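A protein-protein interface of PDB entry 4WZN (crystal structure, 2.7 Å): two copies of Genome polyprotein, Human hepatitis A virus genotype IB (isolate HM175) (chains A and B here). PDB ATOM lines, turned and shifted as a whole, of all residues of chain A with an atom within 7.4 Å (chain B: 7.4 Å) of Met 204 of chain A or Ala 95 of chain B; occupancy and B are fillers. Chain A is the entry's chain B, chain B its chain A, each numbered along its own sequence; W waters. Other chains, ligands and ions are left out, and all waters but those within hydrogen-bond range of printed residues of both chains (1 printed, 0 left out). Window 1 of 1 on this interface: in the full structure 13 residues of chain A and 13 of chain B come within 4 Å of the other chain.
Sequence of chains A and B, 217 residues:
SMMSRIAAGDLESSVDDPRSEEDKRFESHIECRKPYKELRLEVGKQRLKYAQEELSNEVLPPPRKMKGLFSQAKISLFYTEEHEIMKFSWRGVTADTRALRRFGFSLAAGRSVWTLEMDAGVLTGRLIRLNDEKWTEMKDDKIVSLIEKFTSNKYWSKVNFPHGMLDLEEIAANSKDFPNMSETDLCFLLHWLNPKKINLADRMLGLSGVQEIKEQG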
ATOM      1  N   MET A  86      17.772   0.651  27.378  1.00  0.00           N
ATOM      2  CA  MET A  86      19.019   0.566  26.678  1.00  0.00           C
ATOM      3  C   MET A  86      19.105  -0.790  26.092  1.00  0.00           C
ATOM      4  O   MET A  86      19.102  -1.790  26.812  1.00  0.00           O
ATOM      5  CB  MET A  86      20.149   0.819  27.629  1.00  0.00           C
ATOM      6  CG  MET A  86      20.101   2.197  28.103  1.00  0.00           C
ATOM      7  SD  MET A  86      21.550   2.578  29.022  1.00  0.00           S
ATOM      8  CE  MET A  86      21.397   4.283  28.957  1.00  0.00           C
ATOM      9  N   LYS A  87      19.112  -0.830  24.772  1.00  0.00           N
ATOM     10  CA  LYS A  87      19.139  -2.065  24.025  1.00  0.00           C
ATOM     11  C   LYS A  87      20.587  -2.446  23.678  1.00  0.00           C
ATOM     12  O   LYS A  87      21.350  -1.625  23.105  1.00  0.00           O
ATOM     13  CB  LYS A  87      18.260  -1.898  22.762  1.00  0.00           C
ATOM     14  CG  LYS A  87      18.074  -3.130  21.907  1.00  0.00           C
ATOM     15  CD  LYS A  87      17.528  -2.736  20.538  1.00  0.00           C
ATOM     16  CE  LYS A  87      16.555  -3.762  19.965  1.00  0.00           C
ATOM     17  NZ  LYS A  87      16.350  -3.640  18.483  1.00  0.00           N
ATOM     18  N   PHE A  88      20.946  -3.698  24.031  1.00  0.00           N
ATOM     19  CA  PHE A  88      22.250  -4.279  23.716  1.00  0.00           C
ATOM     20  C   PHE A  88      22.127  -5.254  22.576  1.00  0.00           C
ATOM     21  O   PHE A  88      21.457  -6.287  22.718  1.00  0.00           O
ATOM     22  CB  PHE A  88      22.822  -5.019  24.906  1.00  0.00           C
ATOM     23  CG  PHE A  88      23.832  -4.223  25.661  1.00  0.00           C
ATOM     24  CD1 PHE A  88      25.177  -4.279  25.320  1.00  0.00           C
ATOM     25  CD2 PHE A  88      23.450  -3.425  26.725  1.00  0.00           C
ATOM     26  CE1 PHE A  88      26.121  -3.557  26.044  1.00  0.00           C
ATOM     27  CE2 PHE A  88      24.391  -2.746  27.476  1.00  0.00           C
ATOM     28  CZ  PHE A  88      25.721  -2.798  27.124  1.00  0.00           C
ATOM     29  N   SER A  89      22.779  -4.951  21.472  1.00  0.00           N
ATOM     30  CA  SER A  89      22.785  -5.766  20.287  1.00  0.00           C
ATOM     31  C   SER A  89      24.187  -5.728  19.737  1.00  0.00           C
ATOM     32  O   SER A  89      25.115  -5.235  20.401  1.00  0.00           O
ATOM     33  CB  SER A  89      21.769  -5.232  19.278  1.00  0.00           C
ATOM     34  OG  SER A  89      21.786  -3.817  19.139  1.00  0.00           O
ATOM     35  N   ARG A  91      25.065  -3.852  17.468  1.00  0.00           N
ATOM     36  CA  ARG A  91      25.278  -2.426  17.179  1.00  0.00           C
ATOM     37  C   ARG A  91      25.984  -1.724  18.313  1.00  0.00           C
ATOM     38  O   ARG A  91      26.539  -0.642  18.127  1.00  0.00           O
ATOM     39  CB  ARG A  91      23.936  -1.713  16.887  1.00  0.00           C
ATOM     40  CG  ARG A  91      23.038  -2.480  15.935  1.00  0.00           C
ATOM     41  CD  ARG A  91      21.625  -1.963  15.858  1.00  0.00           C
ATOM     42  NE  ARG A  91      21.310  -1.506  14.499  1.00  0.00           N
ATOM     43  CZ  ARG A  91      20.609  -2.200  13.606  1.00  0.00           C
ATOM     44  NH1 ARG A  91      20.132  -3.404  13.912  1.00  0.00           N
ATOM     45  NH2 ARG A  91      20.382  -1.699  12.400  1.00  0.00           N
ATOM     46  N   GLY A  92      25.912  -2.318  19.492  1.00  0.00           N
ATOM     47  CA  GLY A  92      26.453  -1.753  20.718  1.00  0.00           C
ATOM     48  C   GLY A  92      25.320  -1.485  21.675  1.00  0.00           C
ATOM     49  O   GLY A  92      24.413  -2.317  21.796  1.00  0.00           O
ATOM     50  N   VAL A  93      25.344  -0.322  22.344  1.00  0.00           N
ATOM     51  CA  VAL A  93      24.274   0.018  23.305  1.00  0.00           C
ATOM     52  C   VAL A  93      23.526   1.192  22.814  1.00  0.00           C
ATOM     53  O   VAL A  93      24.079   2.286  22.850  1.00  0.00           O
ATOM     54  CB  VAL A  93      24.755   0.363  24.729  1.00  0.00           C
ATOM     55  CG1 VAL A  93      23.614   0.270  25.722  1.00  0.00           C
ATOM     56  CG2 VAL A  93      25.954  -0.462  25.141  1.00  0.00           C
ATOM     57  N   THR A  94      22.245   1.010  22.484  1.00  0.00           N
ATOM     58  CA  THR A  94      21.389   2.123  22.064  1.00  0.00           C
ATOM     59  C   THR A  94      20.482   2.531  23.163  1.00  0.00           C
ATOM     60  O   THR A  94      19.772   1.715  23.720  1.00  0.00           O
ATOM     61  CB  THR A  94      20.556   1.831  20.812  1.00  0.00           C
ATOM     62  OG1 THR A  94      21.320   1.072  19.867  1.00  0.00           O
ATOM     63  CG2 THR A  94      20.048   3.136  20.154  1.00  0.00           C
ATOM     64  N   ALA A  95      20.416   3.799  23.389  1.00  0.00           N
ATOM     65  CA  ALA A  95      19.505   4.442  24.309  1.00  0.00           C
ATOM     66  C   ALA A  95      18.796   5.607  23.570  1.00  0.00           C
ATOM     67  O   ALA A  95      19.165   5.958  22.457  1.00  0.00           O
ATOM     68  CB  ALA A  95      20.274   4.955  25.502  1.00  0.00           C
ATOM     69  N   ASP A  96      17.772   6.165  24.211  1.00  0.00           N
ATOM     70  CA  ASP A  96      16.900   7.253  23.803  1.00  0.00           C
ATOM     71  C   ASP A  96      17.246   8.471  24.664  1.00  0.00           C
ATOM     72  O   ASP A  96      17.172   8.426  25.886  1.00  0.00           O
ATOM     73  CB  ASP A  96      15.436   6.822  24.046  1.00  0.00           C
ATOM     74  CG  ASP A  96      14.370   7.680  23.390  1.00  0.00           C
ATOM     75  OD1 ASP A  96      14.355   8.897  23.636  1.00  0.00           O
ATOM     76  OD2 ASP A  96      13.487   7.114  22.715  1.00  0.00           O
ATOM     77  N   ILE A 198      17.713  11.566  32.771  1.00  0.00           N
ATOM     78  CA  ILE A 198      18.659  10.491  32.994  1.00  0.00           C
ATOM     79  C   ILE A 198      19.905  10.782  32.132  1.00  0.00           C
ATOM     80  O   ILE A 198      19.778  10.955  30.909  1.00  0.00           O
ATOM     81  CB  ILE A 198      18.015   9.118  32.722  1.00  0.00           C
ATOM     82  CG1 ILE A 198      16.977   8.784  33.819  1.00  0.00           C
ATOM     83  CG2 ILE A 198      19.076   8.014  32.588  1.00  0.00           C
ATOM     84  CD1 ILE A 198      15.905   7.783  33.444  1.00  0.00           C
ATOM     85  N   ASN A 199      21.094  10.855  32.775  1.00  0.00           N
ATOM     86  CA  ASN A 199      22.367  11.020  32.091  1.00  0.00           C
ATOM     87  C   ASN A 199      22.698   9.669  31.491  1.00  0.00           C
ATOM     88  O   ASN A 199      23.013   8.717  32.219  1.00  0.00           O
ATOM     89  CB  ASN A 199      23.444  11.426  33.055  1.00  0.00           C
ATOM     90  CG  ASN A 199      24.688  11.993  32.431  1.00  0.00           C
ATOM     91  OD1 ASN A 199      25.303  11.432  31.518  1.00  0.00           O
ATOM     92  ND2 ASN A 199      25.157  13.062  33.023  1.00  0.00           N
ATOM     93  N   LEU A 200      22.580   9.568  30.165  1.00  0.00           N
ATOM     94  CA  LEU A 200      22.810   8.309  29.459  1.00  0.00           C
ATOM     95  C   LEU A 200      24.250   7.783  29.512  1.00  0.00           C
ATOM     96  O   LEU A 200      24.437   6.563  29.555  1.00  0.00           O
ATOM     97  CB  LEU A 200      22.268   8.381  28.020  1.00  0.00           C
ATOM     98  CG  LEU A 200      20.754   8.560  27.918  1.00  0.00           C
ATOM     99  CD1 LEU A 200      20.367   8.982  26.561  1.00  0.00           C
ATOM    100  CD2 LEU A 200      19.988   7.316  28.379  1.00  0.00           C
ATOM    101  N   ALA A 201      25.257   8.688  29.540  1.00  0.00           N
ATOM    102  CA  ALA A 201      26.656   8.272  29.657  1.00  0.00           C
ATOM    103  C   ALA A 201      26.876   7.624  31.018  1.00  0.00           C
ATOM    104  O   ALA A 201      27.550   6.612  31.066  1.00  0.00           O
ATOM    105  CB  ALA A 201      27.600   9.440  29.444  1.00  0.00           C
ATOM    106  N   ASP A 202      26.211   8.110  32.088  1.00  0.00           N
ATOM    107  CA  ASP A 202      26.310   7.499  33.418  1.00  0.00           C
ATOM    108  C   ASP A 202      25.495   6.208  33.511  1.00  0.00           C
ATOM    109  O   ASP A 202      25.920   5.249  34.149  1.00  0.00           O
ATOM    110  CB  ASP A 202      25.854   8.475  34.525  1.00  0.00           C
ATOM    111  CG  ASP A 202      26.701   9.727  34.693  1.00  0.00           C
ATOM    112  OD1 ASP A 202      27.768   9.818  34.037  1.00  0.00           O
ATOM    113  OD2 ASP A 202      26.276  10.637  35.456  1.00  0.00           O
ATOM    114  N   ARG A 203      24.300   6.206  32.929  1.00  0.00           N
ATOM    115  CA  ARG A 203      23.439   5.042  32.959  1.00  0.00           C
ATOM    116  C   ARG A 203      24.052   3.844  32.198  1.00  0.00           C
ATOM    117  O   ARG A 203      23.876   2.719  32.616  1.00  0.00           O
ATOM    118  CB  ARG A 203      22.043   5.419  32.474  1.00  0.00           C
ATOM    119  CG  ARG A 203      21.028   4.291  32.444  1.00  0.00           C
ATOM    120  CD  ARG A 203      20.754   3.686  33.798  1.00  0.00           C
ATOM    121  NE  ARG A 203      19.972   4.556  34.688  1.00  0.00           N
ATOM    122  CZ  ARG A 203      18.649   4.621  34.701  1.00  0.00           C
ATOM    123  NH1 ARG A 203      17.936   3.946  33.809  1.00  0.00           N
ATOM    124  NH2 ARG A 203      18.027   5.368  35.597  1.00  0.00           N
ATOM    125  N   MET A 204      24.846   4.087  31.167  1.00  0.00           N
ATOM    126  CA  MET A 204      25.549   3.034  30.425  1.00  0.00           C
ATOM    127  C   MET A 204      26.703   2.474  31.280  1.00  0.00           C
ATOM    128  O   MET A 204      27.139   1.342  31.068  1.00  0.00           O
ATOM    129  CB  MET A 204      26.064   3.565  29.087  1.00  0.00           C
ATOM    130  CG  MET A 204      24.968   3.823  28.106  1.00  0.00           C
ATOM    131  SD  MET A 204      25.583   4.525  26.568  1.00  0.00           S
ATOM    132  CE  MET A 204      24.017   4.844  25.609  1.00  0.00           C
ATOM    133  N   LEU A 205      27.157   3.259  32.279  1.00  0.00           N
ATOM    134  CA  LEU A 205      28.207   2.904  33.230  1.00  0.00           C
ATOM    135  C   LEU A 205      27.581   2.347  34.531  1.00  0.00           C
ATOM    136  O   LEU A 205      28.262   2.202  35.547  1.00  0.00           O
ATOM    137  CB  LEU A 205      29.133   4.123  33.464  1.00  0.00           C
ATOM    138  CG  LEU A 205      29.991   4.554  32.213  1.00  0.00           C
ATOM    139  CD1 LEU A 205      30.450   5.995  32.313  1.00  0.00           C
ATOM    140  CD2 LEU A 205      31.190   3.599  31.965  1.00  0.00           C
ATOM    141  N   GLY A 206      26.277   2.020  34.445  1.00  0.00           N
ATOM    142  CA  GLY A 206      25.455   1.443  35.502  1.00  0.00           C
ATOM    143  C   GLY A 206      25.152   2.346  36.677  1.00  0.00           C
ATOM    144  O   GLY A 206      24.897   1.857  37.782  1.00  0.00           O
ATOM    145  N   LEU A 207      25.168   3.667  36.455  1.00  0.00           N
ATOM    146  CA  LEU A 207      24.860   4.654  37.504  1.00  0.00           C
ATOM    147  C   LEU A 207      23.404   5.143  37.294  1.00  0.00           C
ATOM    148  O   LEU A 207      22.913   5.042  36.169  1.00  0.00           O
ATOM    149  CB  LEU A 207      25.869   5.829  37.457  1.00  0.00           C
ATOM    150  CG  LEU A 207      27.360   5.462  37.412  1.00  0.00           C
ATOM    151  CD1 LEU A 207      28.181   6.587  36.839  1.00  0.00           C
ATOM    152  CD2 LEU A 207      27.875   5.079  38.772  1.00  0.00           C
ATOM    153  N   GLU B  81      35.821   7.345  34.217  1.00  0.00           N
ATOM    154  CA  GLU B  81      35.357   6.509  33.121  1.00  0.00           C
ATOM    155  C   GLU B  81      34.810   7.363  31.988  1.00  0.00           C
ATOM    156  O   GLU B  81      34.275   8.449  32.239  1.00  0.00           O
ATOM    157  CB  GLU B  81      34.335   5.497  33.618  1.00  0.00           C
ATOM    158  CG  GLU B  81      34.919   4.524  34.623  1.00  0.00           C
ATOM    159  CD  GLU B  81      33.990   3.401  35.017  1.00  0.00           C
ATOM    160  OE1 GLU B  81      32.752   3.610  35.043  1.00  0.00           O
ATOM    161  OE2 GLU B  81      34.516   2.309  35.332  1.00  0.00           O
ATOM    162  N   HIS B  83      33.196   7.338  27.563  1.00  0.00           N
ATOM    163  CA  HIS B  83      32.829   6.735  26.270  1.00  0.00           C
ATOM    164  C   HIS B  83      33.694   7.495  25.254  1.00  0.00           C
ATOM    165  O   HIS B  83      33.592   8.723  25.171  1.00  0.00           O
ATOM    166  CB  HIS B  83      31.327   6.931  25.942  1.00  0.00           C
ATOM    167  CG  HIS B  83      30.425   6.314  26.953  1.00  0.00           C
ATOM    168  ND1 HIS B  83      30.216   4.946  26.992  1.00  0.00           N
ATOM    169  CD2 HIS B  83      29.770   6.885  27.987  1.00  0.00           C
ATOM    170  CE1 HIS B  83      29.417   4.736  28.022  1.00  0.00           C
ATOM    171  NE2 HIS B  83      29.122   5.871  28.650  1.00  0.00           N
ATOM    172  N   GLU B  84      34.595   6.793  24.547  1.00  0.00           N
ATOM    173  CA  GLU B  84      35.491   7.430  23.552  1.00  0.00           C
ATOM    174  C   GLU B  84      34.730   7.815  22.253  1.00  0.00           C
ATOM    175  O   GLU B  84      35.137   8.734  21.551  1.00  0.00           O
ATOM    176  CB  GLU B  84      36.678   6.508  23.229  1.00  0.00           C
ATOM    177  CG  GLU B  84      37.539   6.126  24.424  1.00  0.00           C
ATOM    178  CD  GLU B  84      38.434   4.918  24.186  1.00  0.00           C
ATOM    179  OE1 GLU B  84      37.933   3.772  24.291  1.00  0.00           O
ATOM    180  OE2 GLU B  84      39.635   5.118  23.878  1.00  0.00           O
ATOM    181  N   ILE B  85      33.632   7.089  21.943  1.00  0.00           N
ATOM    182  CA  ILE B  85      32.740   7.282  20.796  1.00  0.00           C
ATOM    183  C   ILE B  85      31.263   7.172  21.252  1.00  0.00           C
ATOM    184  O   ILE B  85      30.906   6.300  22.061  1.00  0.00           O
ATOM    185  CB  ILE B  85      33.077   6.313  19.610  1.00  0.00           C
ATOM    186  CG1 ILE B  85      34.460   6.613  19.007  1.00  0.00           C
ATOM    187  CG2 ILE B  85      32.042   6.398  18.502  1.00  0.00           C
ATOM    188  CD1 ILE B  85      35.607   5.676  19.474  1.00  0.00           C
ATOM    189  N   MET B  86      30.437   8.090  20.743  1.00  0.00           N
ATOM    190  CA  MET B  86      28.991   8.170  20.906  1.00  0.00           C
ATOM    191  C   MET B  86      28.515   8.436  19.490  1.00  0.00           C
ATOM    192  O   MET B  86      29.097   9.278  18.810  1.00  0.00           O
ATOM    193  CB  MET B  86      28.532   9.335  21.821  1.00  0.00           C
ATOM    194  CG  MET B  86      28.763   9.168  23.285  1.00  0.00           C
ATOM    195  SD  MET B  86      27.896   7.716  23.905  1.00  0.00           S
ATOM    196  CE  MET B  86      27.232   8.376  25.556  1.00  0.00           C
ATOM    197  N   LYS B  87      27.474   7.694  19.036  1.00  0.00           N
ATOM    198  CA  LYS B  87      26.875   7.832  17.699  1.00  0.00           C
ATOM    199  C   LYS B  87      25.446   8.267  17.867  1.00  0.00           C
ATOM    200  O   LYS B  87      24.652   7.601  18.528  1.00  0.00           O
ATOM    201  CB  LYS B  87      26.986   6.558  16.866  1.00  0.00           C
ATOM    202  CG  LYS B  87      28.375   6.305  16.410  1.00  0.00           C
ATOM    203  CD  LYS B  87      28.499   4.955  15.795  1.00  0.00           C
ATOM    204  CE  LYS B  87      29.848   4.822  15.119  1.00  0.00           C
ATOM    205  NZ  LYS B  87      30.023   3.499  14.450  1.00  0.00           N
ATOM    206  N   VAL B  93      21.011   7.553  20.922  1.00  0.00           N
ATOM    207  CA  VAL B  93      22.475   7.456  21.050  1.00  0.00           C
ATOM    208  C   VAL B  93      22.900   5.984  21.135  1.00  0.00           C
ATOM    209  O   VAL B  93      22.201   5.196  21.736  1.00  0.00           O
ATOM    210  CB  VAL B  93      23.031   8.314  22.234  1.00  0.00           C
ATOM    211  CG1 VAL B  93      22.495   7.838  23.575  1.00  0.00           C
ATOM    212  CG2 VAL B  93      24.557   8.329  22.247  1.00  0.00           C
ATOM    213  N   THR B  94      24.021   5.630  20.519  1.00  0.00           N
ATOM    214  CA  THR B  94      24.613   4.285  20.480  1.00  0.00           C
ATOM    215  C   THR B  94      26.067   4.390  20.938  1.00  0.00           C
ATOM    216  O   THR B  94      26.844   5.160  20.384  1.00  0.00           O
ATOM    217  CB  THR B  94      24.544   3.721  19.037  1.00  0.00           C
ATOM    218  OG1 THR B  94      23.198   3.762  18.581  1.00  0.00           O
ATOM    219  CG2 THR B  94      25.062   2.312  18.921  1.00  0.00           C
ATOM    220  N   ALA B  95      26.429   3.635  21.959  1.00  0.00           N
ATOM    221  CA  ALA B  95      27.809   3.598  22.430  1.00  0.00           C
ATOM    222  C   ALA B  95      28.402   2.225  22.157  1.00  0.00           C
ATOM    223  O   ALA B  95      27.656   1.282  21.899  1.00  0.00           O
ATOM    224  CB  ALA B  95      27.879   3.908  23.908  1.00  0.00           C
ATOM    225  N   ASP B  96      29.754   2.120  22.188  1.00  0.00           N
ATOM    226  CA  ASP B  96      30.485   0.854  22.031  1.00  0.00           C
ATOM    227  C   ASP B  96      30.209  -0.022  23.279  1.00  0.00           C
ATOM    228  O   ASP B  96      30.148   0.500  24.406  1.00  0.00           O
ATOM    229  CB  ASP B  96      32.019   1.097  21.966  1.00  0.00           C
ATOM    230  CG  ASP B  96      32.603   1.577  20.643  1.00  0.00           C
ATOM    231  OD1 ASP B  96      31.987   1.296  19.578  1.00  0.00           O
ATOM    232  OD2 ASP B  96      33.713   2.178  20.662  1.00  0.00           O
ATOM    233  N   THR B  97      30.109  -1.359  23.069  1.00  0.00           N
ATOM    234  CA  THR B  97      30.003  -2.391  24.107  1.00  0.00           C
ATOM    235  C   THR B  97      31.099  -2.155  25.188  1.00  0.00           C
ATOM    236  O   THR B  97      30.834  -2.361  26.363  1.00  0.00           O
ATOM    237  CB  THR B  97      30.134  -3.748  23.424  1.00  0.00           C
ATOM    238  OG1 THR B  97      29.029  -3.892  22.521  1.00  0.00           O
ATOM    239  CG2 THR B  97      30.197  -4.924  24.415  1.00  0.00           C
ATOM    240  N   ARG B  98      32.284  -1.638  24.782  1.00  0.00           N
ATOM    241  CA  ARG B  98      33.419  -1.311  25.646  1.00  0.00           C
ATOM    242  C   ARG B  98      33.763   0.181  25.745  1.00  0.00           C
ATOM    243  O   ARG B  98      34.135   0.787  24.740  1.00  0.00           O
ATOM    244  CB  ARG B  98      34.680  -2.112  25.269  1.00  0.00           C
ATOM    245  CG  ARG B  98      34.588  -3.605  25.570  1.00  0.00           C
ATOM    246  CD  ARG B  98      35.921  -4.265  25.359  1.00  0.00           C
ATOM    247  NE  ARG B  98      36.560  -3.819  24.119  1.00  0.00           N
ATOM    248  CZ  ARG B  98      37.805  -4.118  23.766  1.00  0.00           C
ATOM    249  NH1 ARG B  98      38.560  -4.878  24.551  1.00  0.00           N
ATOM    250  NH2 ARG B  98      38.304  -3.662  22.623  1.00  0.00           N
ATOM    251  N   ALA B  99      33.668   0.746  26.982  1.00  0.00           N
ATOM    252  CA  ALA B  99      34.058   2.115  27.356  1.00  0.00           C
ATOM    253  C   ALA B  99      35.489   2.071  27.932  1.00  0.00           C
ATOM    254  O   ALA B  99      36.127   1.006  27.981  1.00  0.00           O
ATOM    255  CB  ALA B  99      33.106   2.682  28.404  1.00  0.00           C
ATOM    256  N   ILE B 198      36.250  -1.157  29.557  1.00  0.00           N
ATOM    257  CA  ILE B 198      35.110  -1.557  30.405  1.00  0.00           C
ATOM    258  C   ILE B 198      34.055  -2.226  29.497  1.00  0.00           C
ATOM    259  O   ILE B 198      33.572  -1.560  28.579  1.00  0.00           O
ATOM    260  CB  ILE B 198      34.400  -0.317  31.102  1.00  0.00           C
ATOM    261  CG1 ILE B 198      35.338   0.588  31.867  1.00  0.00           C
ATOM    262  CG2 ILE B 198      33.265  -0.750  32.015  1.00  0.00           C
ATOM    263  CD1 ILE B 198      34.850   1.990  31.893  1.00  0.00           C
ATOM    264  N   ASN B 199      33.598  -3.460  29.824  1.00  0.00           N
ATOM    265  CA  ASN B 199      32.490  -4.059  29.076  1.00  0.00           C
ATOM    266  C   ASN B 199      31.181  -3.586  29.721  1.00  0.00           C
ATOM    267  O   ASN B 199      30.824  -4.019  30.815  1.00  0.00           O
ATOM    268  CB  ASN B 199      32.548  -5.605  29.012  1.00  0.00           C
ATOM    269  CG  ASN B 199      31.542  -6.166  28.004  1.00  0.00           C
ATOM    270  OD1 ASN B 199      30.346  -5.793  27.953  1.00  0.00           O
ATOM    271  ND2 ASN B 199      32.013  -7.027  27.130  1.00  0.00           N
ATOM    272  N   LEU B 200      30.453  -2.728  29.022  1.00  0.00           N
ATOM    273  CA  LEU B 200      29.191  -2.162  29.498  1.00  0.00           C
ATOM    274  C   LEU B 200      28.090  -3.183  29.728  1.00  0.00           C
ATOM    275  O   LEU B 200      27.349  -3.045  30.700  1.00  0.00           O
ATOM    276  CB  LEU B 200      28.722  -1.023  28.597  1.00  0.00           C
ATOM    277  CG  LEU B 200      29.701   0.127  28.383  1.00  0.00           C
ATOM    278  CD1 LEU B 200      29.090   1.149  27.490  1.00  0.00           C
ATOM    279  CD2 LEU B 200      30.178   0.721  29.733  1.00  0.00           C
ATOM    280  N   ALA B 201      28.001  -4.232  28.887  1.00  0.00           N
ATOM    281  CA  ALA B 201      27.001  -5.285  29.096  1.00  0.00           C
ATOM    282  C   ALA B 201      27.262  -5.986  30.437  1.00  0.00           C
ATOM    283  O   ALA B 201      26.335  -6.068  31.235  1.00  0.00           O
ATOM    284  CB  ALA B 201      27.019  -6.280  27.950  1.00  0.00           C
ATOM    285  N   ARG B 203      28.882  -4.668  32.877  1.00  0.00           N
ATOM    286  CA  ARG B 203      28.705  -3.572  33.825  1.00  0.00           C
ATOM    287  C   ARG B 203      27.240  -3.425  34.256  1.00  0.00           C
ATOM    288  O   ARG B 203      26.934  -3.358  35.452  1.00  0.00           O
ATOM    289  CB  ARG B 203      29.300  -2.270  33.231  1.00  0.00           C
ATOM    290  CG  ARG B 203      28.961  -0.958  33.942  1.00  0.00           C
ATOM    291  CD  ARG B 203      29.384  -0.929  35.405  1.00  0.00           C
ATOM    292  NE  ARG B 203      30.827  -1.046  35.571  1.00  0.00           N
ATOM    293  CZ  ARG B 203      31.672  -0.037  35.428  1.00  0.00           C
ATOM    294  NH1 ARG B 203      31.223   1.171  35.114  1.00  0.00           N
ATOM    295  NH2 ARG B 203      32.975  -0.228  35.592  1.00  0.00           N
ATOM    296  N   MET B 204      26.342  -3.437  33.278  1.00  0.00           N
ATOM    297  CA  MET B 204      24.914  -3.276  33.477  1.00  0.00           C
ATOM    298  C   MET B 204      24.245  -4.461  34.063  1.00  0.00           C
ATOM    299  O   MET B 204      23.094  -4.360  34.480  1.00  0.00           O
ATOM    300  CB  MET B 204      24.267  -2.858  32.170  1.00  0.00           C
ATOM    301  CG  MET B 204      24.528  -1.414  31.868  1.00  0.00           C
ATOM    302  SD  MET B 204      23.683  -1.007  30.362  1.00  0.00           S
ATOM    303  CE  MET B 204      24.990  -0.522  29.412  1.00  0.00           C
HETATM  304  O   HOH W   1      21.790   0.254  33.249  1.00  0.00           O
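The backbone carbonyl oxygen of Ala 201 of chain A lies within hydrogen-bond range of a ring nitrogen (NE2) of His 83 of chain B (3.0 Å).
The backbone carbonyl oxygen (O) of Val 93 of chain B is in hydrogen-bond range of the backbone NH (N) of Ala 95 of chain A (2.8 Å).
The backbone carbonyl oxygen of Ala 95 of chain B lies within hydrogen-bond range of the backbone NH of Val 93 of chain A.
O of Leu 205 of chain A lies within hydrogen-bond range of NH1 of Arg 203 of chain B.
The side-chain carboxylate of Glu 81 of chain B lies within salt-bridge range of the guanidinium group of Arg 203 of chain B.
N of Ala 201 of chain B sits at hydrogen-bond distance from OD1 of Asn 199 of chain B (3.0 Å).
The backbone NH (N) of Lys 87 of chain A lies within hydrogen-bond range of the backbone carbonyl oxygen (O) of Thr 94 of chain A (2.8 Å).
CE2 of Phe 88 of chain A touches CE of Met 204 of chain B, 3.0 Å away.
Gly 92 of chain A touches Ala 95 of chain B (CA to O, 3.5 Å).
Val 93 of chain A touches Val 93 of chain B.
Val 93 of chain B touches Thr 94 of chain A.
Thr 94 of chain A touches Thr 94 of chain B.
Val 93 of chain B touches Leu 200 of chain A (CG1 to CD1, 3.8 Å).
Val 93 of chain B touches Met 204 of chain A.
Of the printed residues of chain B, Met 204 of chain A touches His 83 (3.7 Å), Val 93 (3.9 Å), Ala 95 (3.6 Å), Leu 200 (3.4 Å) and Met 204 (3.3 Å).
Of chain A, only Gly 92, Val 93 and Met 204 come within 4 Å of Ala 95 of chain B.
Of the printed residues of chain B, Ala 201 of chain A touches His 83 (3.0 Å).
Of the printed residues of chain A, His 83 of chain B touches Ala 201 (3.0 Å), Met 204 (3.7 Å) and Leu 205 (3.9 Å).
The nearest residue of chain B that does not touch Met 204 of chain A is Arg 203 of chain B (4.1 Å).
The nearest printed residue of chain A that does not touch Met 204 of chain B is Val 93 of chain A (4.02 Å).
Of the 19 printed residues of chain B, 11 touch a printed residue of chain A.
Printed residues of chain B that touch a printed residue of chain A: Glu 81, His 83, Val 93, Thr 94, Ala 95, Thr 97, Ile 198, Leu 200, Ala 201, Arg 203 and Met 204.
Hydrophobic or aromatic side chains of chain B within 4 Å of the printed part of chain A: His 83, Val 93, Ala 95, Ile 198, Leu 200, Ala 201 and Met 204.
Hydrophobic or aromatic side chains of chain A within 4 Å of the printed part of chain B: Phe 88, Leu 200, Ala 201, Met 204 and Leu 205.
Val 93 of chain A touches Thr 94 of chain B, and with the chains exchanged Thr 94 of chain A touches Val 93 of chain B.
Met 204 of chain A touches Val 93 of chain B, but with the chains exchanged Val 93 of chain A does not touch Met 204 of chain B (4.02 Å).
Of the 24 pairs that touch across the chains among the printed residues, 7 have their exchanged pair printed and touching as well.
Water W1 lies within hydrogen-bond range of O of Arg 203 of chain A (3.3 Å) and SD of Met 204 of chain B (3.7 Å).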
